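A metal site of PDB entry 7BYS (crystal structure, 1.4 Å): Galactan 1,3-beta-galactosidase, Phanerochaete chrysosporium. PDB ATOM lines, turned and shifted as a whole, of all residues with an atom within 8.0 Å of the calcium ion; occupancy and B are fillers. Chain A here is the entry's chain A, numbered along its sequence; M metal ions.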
ATOM      1  N   TYR A 307      -4.685  21.565   0.419  1.00  0.00           N
ATOM      2  CA  TYR A 307      -4.060  22.152  -0.759  1.00  0.00           C
ATOM      3  C   TYR A 307      -4.749  21.570  -1.981  1.00  0.00           C
ATOM      4  O   TYR A 307      -4.742  20.354  -2.169  1.00  0.00           O
ATOM      5  CB  TYR A 307      -2.563  21.800  -0.819  1.00  0.00           C
ATOM      6  CG  TYR A 307      -1.770  22.285   0.379  1.00  0.00           C
ATOM      7  CD1 TYR A 307      -1.694  21.528   1.542  1.00  0.00           C
ATOM      8  CD2 TYR A 307      -1.067  23.495   0.336  1.00  0.00           C
ATOM      9  CE1 TYR A 307      -0.952  21.957   2.636  1.00  0.00           C
ATOM     10  CE2 TYR A 307      -0.332  23.929   1.425  1.00  0.00           C
ATOM     11  CZ  TYR A 307      -0.281  23.156   2.570  1.00  0.00           C
ATOM     12  OH  TYR A 307       0.453  23.590   3.659  1.00  0.00           O
ATOM     13  N   GLU A 308      -5.287  22.431  -2.835  1.00  0.00           N
ATOM     14  CA  GLU A 308      -5.946  21.979  -4.052  1.00  0.00           C
ATOM     15  C   GLU A 308      -4.914  21.599  -5.105  1.00  0.00           C
ATOM     16  O   GLU A 308      -3.953  22.345  -5.335  1.00  0.00           O
ATOM     17  CB  GLU A 308      -6.858  23.077  -4.611  1.00  0.00           C
ATOM     18  CG  GLU A 308      -8.001  23.470  -3.688  1.00  0.00           C
ATOM     19  CD  GLU A 308      -9.041  22.372  -3.489  1.00  0.00           C
ATOM     20  OE1 GLU A 308      -9.153  21.466  -4.333  1.00  0.00           O
ATOM     21  OE2 GLU A 308      -9.748  22.426  -2.465  1.00  0.00           O
ATOM     22  N   ALA A 309      -5.105  20.441  -5.739  1.00  0.00           N
ATOM     23  CA  ALA A 309      -4.171  20.018  -6.773  1.00  0.00           C
ATOM     24  C   ALA A 309      -4.108  21.021  -7.915  1.00  0.00           C
ATOM     25  O   ALA A 309      -3.037  21.261  -8.487  1.00  0.00           O
ATOM     26  CB  ALA A 309      -4.571  18.638  -7.304  1.00  0.00           C
ATOM     27  N   GLU A 310      -5.256  21.628  -8.256  1.00  0.00           N
ATOM     28  CA  GLU A 310      -5.314  22.545  -9.387  1.00  0.00           C
ATOM     29  C   GLU A 310      -4.564  23.838  -9.131  1.00  0.00           C
ATOM     30  O   GLU A 310      -4.299  24.573 -10.084  1.00  0.00           O
ATOM     31  CB  GLU A 310      -6.772  22.796  -9.792  1.00  0.00           C
ATOM     32  CG  GLU A 310      -7.637  23.431  -8.707  1.00  0.00           C
ATOM     33  CD  GLU A 310      -8.328  22.412  -7.802  1.00  0.00           C
ATOM     34  OE1 GLU A 310      -7.845  21.253  -7.695  1.00  0.00           O
ATOM     35  OE2 GLU A 310      -9.369  22.778  -7.238  1.00  0.00           O
ATOM     36  N   ASN A 311      -4.214  24.136  -7.880  1.00  0.00           N
ATOM     37  CA  ASN A 311      -3.376  25.271  -7.563  1.00  0.00           C
ATOM     38  C   ASN A 311      -1.895  24.914  -7.583  1.00  0.00           C
ATOM     39  O   ASN A 311      -1.046  25.806  -7.382  1.00  0.00           O
ATOM     40  CB  ASN A 311      -3.761  25.864  -6.207  1.00  0.00           C
ATOM     41  CG  ASN A 311      -5.129  26.508  -6.227  1.00  0.00           C
ATOM     42  OD1 ASN A 311      -5.592  26.952  -7.282  1.00  0.00           O
ATOM     43  ND2 ASN A 311      -5.776  26.562  -5.066  1.00  0.00           N
ATOM     44  N   LEU A 321      -9.237  19.411 -14.859  1.00  0.00           N
ATOM     45  CA  LEU A 321     -10.570  18.874 -15.116  1.00  0.00           C
ATOM     46  C   LEU A 321     -11.575  19.568 -14.214  1.00  0.00           C
ATOM     47  O   LEU A 321     -11.253  19.973 -13.101  1.00  0.00           O
ATOM     48  CB  LEU A 321     -10.613  17.377 -14.800  1.00  0.00           C
ATOM     49  CG  LEU A 321      -9.578  16.548 -15.554  1.00  0.00           C
ATOM     50  CD1 LEU A 321      -9.767  15.069 -15.312  1.00  0.00           C
ATOM     51  CD2 LEU A 321      -9.595  16.876 -17.050  1.00  0.00           C
ATOM     52  N   GLY A 323     -15.493  19.296 -12.404  1.00  0.00           N
ATOM     53  CA  GLY A 323     -16.513  18.361 -12.010  1.00  0.00           C
ATOM     54  C   GLY A 323     -17.117  18.719 -10.670  1.00  0.00           C
ATOM     55  O   GLY A 323     -16.430  19.226  -9.785  1.00  0.00           O
ATOM     56  N   GLY A 325     -18.034  16.808  -8.314  1.00  0.00           N
ATOM     57  CA  GLY A 325     -17.580  16.012  -7.191  1.00  0.00           C
ATOM     58  C   GLY A 325     -16.262  16.421  -6.593  1.00  0.00           C
ATOM     59  O   GLY A 325     -15.821  15.808  -5.615  1.00  0.00           O
ATOM     60  N   PHE A 326     -15.615  17.448  -7.142  1.00  0.00           N
ATOM     61  CA  PHE A 326     -14.286  17.900  -6.742  1.00  0.00           C
ATOM     62  C   PHE A 326     -14.364  19.128  -5.847  1.00  0.00           C
ATOM     63  O   PHE A 326     -15.149  20.050  -6.096  1.00  0.00           O
ATOM     64  CB  PHE A 326     -13.451  18.318  -7.949  1.00  0.00           C
ATOM     65  CG  PHE A 326     -13.278  17.271  -8.983  1.00  0.00           C
ATOM     66  CD1 PHE A 326     -13.056  15.950  -8.636  1.00  0.00           C
ATOM     67  CD2 PHE A 326     -13.301  17.600 -10.328  1.00  0.00           C
ATOM     68  CE1 PHE A 326     -12.887  14.975  -9.613  1.00  0.00           C
ATOM     69  CE2 PHE A 326     -13.133  16.642 -11.306  1.00  0.00           C
ATOM     70  CZ  PHE A 326     -12.927  15.333 -10.944  1.00  0.00           C
ATOM     71  N   SER A 327     -13.486  19.170  -4.852  1.00  0.00           N
ATOM     72  CA  SER A 327     -13.297  20.392  -4.090  1.00  0.00           C
ATOM     73  C   SER A 327     -12.783  21.493  -5.021  1.00  0.00           C
ATOM     74  O   SER A 327     -11.909  21.248  -5.872  1.00  0.00           O
ATOM     75  CB  SER A 327     -12.279  20.127  -2.975  1.00  0.00           C
ATOM     76  OG  SER A 327     -11.976  21.327  -2.280  1.00  0.00           O
ATOM     77  N   GLY A 328     -13.339  22.686  -4.886  1.00  0.00           N
ATOM     78  CA  GLY A 328     -13.037  23.757  -5.802  1.00  0.00           C
ATOM     79  C   GLY A 328     -13.583  23.556  -7.196  1.00  0.00           C
ATOM     80  O   GLY A 328     -13.320  24.388  -8.072  1.00  0.00           O
ATOM     81  N   GLY A 329     -14.336  22.492  -7.426  1.00  0.00           N
ATOM     82  CA  GLY A 329     -14.874  22.209  -8.731  1.00  0.00           C
ATOM     83  C   GLY A 329     -13.858  21.725  -9.743  1.00  0.00           C
ATOM     84  O   GLY A 329     -14.200  21.593 -10.919  1.00  0.00           O
ATOM     85  N   LYS A 330     -12.627  21.449  -9.316  1.00  0.00           N
ATOM     86  CA  LYS A 330     -11.549  21.154 -10.250  1.00  0.00           C
ATOM     87  C   LYS A 330     -10.620  20.094  -9.678  1.00  0.00           C
ATOM     88  O   LYS A 330     -10.503  19.934  -8.464  1.00  0.00           O
ATOM     89  CB  LYS A 330     -10.721  22.413 -10.567  1.00  0.00           C
ATOM     90  CG  LYS A 330     -11.528  23.501 -11.269  1.00  0.00           C
ATOM     91  CD  LYS A 330     -10.689  24.693 -11.648  1.00  0.00           C
ATOM     92  CE  LYS A 330     -11.561  25.755 -12.301  1.00  0.00           C
ATOM     93  NZ  LYS A 330     -12.680  25.140 -13.091  1.00  0.00           N
ATOM     94  N   ALA A 331      -9.967  19.368 -10.584  1.00  0.00           N
ATOM     95  CA  ALA A 331      -8.957  18.379 -10.222  1.00  0.00           C
ATOM     96  C   ALA A 331      -7.884  18.408 -11.293  1.00  0.00           C
ATOM     97  O   ALA A 331      -8.039  19.055 -12.331  1.00  0.00           O
ATOM     98  CB  ALA A 331      -9.565  16.974 -10.088  1.00  0.00           C
ATOM     99  N   VAL A 332      -6.808  17.667 -11.063  1.00  0.00           N
ATOM    100  CA  VAL A 332      -5.740  17.520 -12.037  1.00  0.00           C
ATOM    101  C   VAL A 332      -5.854  16.126 -12.654  1.00  0.00           C
ATOM    102  O   VAL A 332      -5.810  15.116 -11.938  1.00  0.00           O
ATOM    103  CB  VAL A 332      -4.358  17.755 -11.423  1.00  0.00           C
ATOM    104  CG1 VAL A 332      -3.257  17.447 -12.444  1.00  0.00           C
ATOM    105  CG2 VAL A 332      -4.237  19.195 -10.954  1.00  0.00           C
ATOM    106  N   TYR A 358      -6.941  13.056  -1.941  1.00  0.00           N
ATOM    107  CA  TYR A 358      -8.322  13.007  -2.433  1.00  0.00           C
ATOM    108  C   TYR A 358      -8.297  12.891  -3.947  1.00  0.00           C
ATOM    109  O   TYR A 358      -7.723  13.754  -4.634  1.00  0.00           O
ATOM    110  CB  TYR A 358      -9.092  14.249  -1.998  1.00  0.00           C
ATOM    111  CG  TYR A 358      -9.491  14.225  -0.546  1.00  0.00           C
ATOM    112  CD1 TYR A 358      -8.539  14.372   0.466  1.00  0.00           C
ATOM    113  CD2 TYR A 358     -10.817  14.074  -0.184  1.00  0.00           C
ATOM    114  CE1 TYR A 358      -8.913  14.321   1.815  1.00  0.00           C
ATOM    115  CE2 TYR A 358     -11.198  14.032   1.143  1.00  0.00           C
ATOM    116  CZ  TYR A 358     -10.240  14.145   2.133  1.00  0.00           C
ATOM    117  OH  TYR A 358     -10.648  14.106   3.442  1.00  0.00           O
ATOM    118  N   VAL A 392     -15.118  11.321  -5.372  1.00  0.00           N
ATOM    119  CA  VAL A 392     -13.816  11.469  -4.727  1.00  0.00           C
ATOM    120  C   VAL A 392     -13.814  10.695  -3.410  1.00  0.00           C
ATOM    121  O   VAL A 392     -14.776  10.783  -2.629  1.00  0.00           O
ATOM    122  CB  VAL A 392     -13.480  12.955  -4.506  1.00  0.00           C
ATOM    123  CG1 VAL A 392     -12.244  13.128  -3.597  1.00  0.00           C
ATOM    124  CG2 VAL A 392     -13.277  13.629  -5.855  1.00  0.00           C
ATOM    125  N   LEU A 421      -6.362  13.831  -9.349  1.00  0.00           N
ATOM    126  CA  LEU A 421      -6.081  14.325  -8.006  1.00  0.00           C
ATOM    127  C   LEU A 421      -6.862  15.604  -7.742  1.00  0.00           C
ATOM    128  O   LEU A 421      -6.705  16.603  -8.457  1.00  0.00           O
ATOM    129  CB  LEU A 421      -4.586  14.559  -7.820  1.00  0.00           C
ATOM    130  CG  LEU A 421      -4.130  14.842  -6.375  1.00  0.00           C
ATOM    131  CD1 LEU A 421      -4.310  13.619  -5.464  1.00  0.00           C
ATOM    132  CD2 LEU A 421      -2.684  15.301  -6.360  1.00  0.00           C
ATOM    133  N   ASP A 422      -7.705  15.588  -6.709  1.00  0.00           N
ATOM    134  CA  ASP A 422      -8.565  16.697  -6.338  1.00  0.00           C
ATOM    135  C   ASP A 422      -7.846  17.668  -5.401  1.00  0.00           C
ATOM    136  O   ASP A 422      -7.801  18.871  -5.668  1.00  0.00           O
ATOM    137  CB  ASP A 422      -9.822  16.151  -5.658  1.00  0.00           C
ATOM    138  CG  ASP A 422     -10.820  17.219  -5.288  1.00  0.00           C
ATOM    139  OD1 ASP A 422     -10.630  18.390  -5.635  1.00  0.00           O
ATOM    140  OD2 ASP A 422     -11.825  16.879  -4.628  1.00  0.00           O
ATOM    141  N   LYS A 423      -7.317  17.150  -4.293  1.00  0.00           N
ATOM    142  CA  LYS A 423      -6.631  17.953  -3.294  1.00  0.00           C
ATOM    143  C   LYS A 423      -5.897  16.997  -2.374  1.00  0.00           C
ATOM    144  O   LYS A 423      -6.062  15.777  -2.458  1.00  0.00           O
ATOM    145  CB  LYS A 423      -7.604  18.820  -2.471  1.00  0.00           C
ATOM    146  CG  LYS A 423      -8.655  18.030  -1.684  1.00  0.00           C
ATOM    147  CD  LYS A 423      -9.374  18.940  -0.702  1.00  0.00           C
ATOM    148  CE  LYS A 423     -10.245  18.145   0.244  1.00  0.00           C
ATOM    149  NZ  LYS A 423     -10.694  19.010   1.378  1.00  0.00           N
ATOM    150  N   ILE A 424      -5.072  17.556  -1.497  1.00  0.00           N
ATOM    151  CA  ILE A 424      -4.441  16.814  -0.415  1.00  0.00           C
ATOM    152  C   ILE A 424      -4.735  17.545   0.886  1.00  0.00           C
ATOM    153  O   ILE A 424      -4.969  18.761   0.899  1.00  0.00           O
ATOM    154  CB  ILE A 424      -2.917  16.597  -0.601  1.00  0.00           C
ATOM    155  CG1 ILE A 424      -2.127  17.906  -0.427  1.00  0.00           C
ATOM    156  CG2 ILE A 424      -2.621  15.956  -1.958  1.00  0.00           C
ATOM    157  CD1 ILE A 424      -0.610  17.719  -0.472  1.00  0.00           C
HETATM  158 CA    CA M   1      -9.716  20.416  -6.307  1.00  0.00          CA
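Within 4 Å of the calcium ion: Glu 308, Glu 310, Ser 327, Lys 330 and Asp 422.
The calcium ion is bound by OE1 of Glu 308 (2.3 Å), OD1 of Asp 422 (2.3 Å), O of Lys 330 (2.3 Å), O of Ser 327 (2.4 Å), OE1 of Glu 310 (2.5 Å), O of Asp 422 (2.5 Å) and OE2 of Glu 310 (2.6 Å).
The backbone carbonyl oxygen of Asp 422 sits close to the backbone NH of Ala 309.
The backbone NH of Asp 422 sits at hydrogen-bond distance from the backbone carbonyl oxygen of Tyr 358 (2.8 Å).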
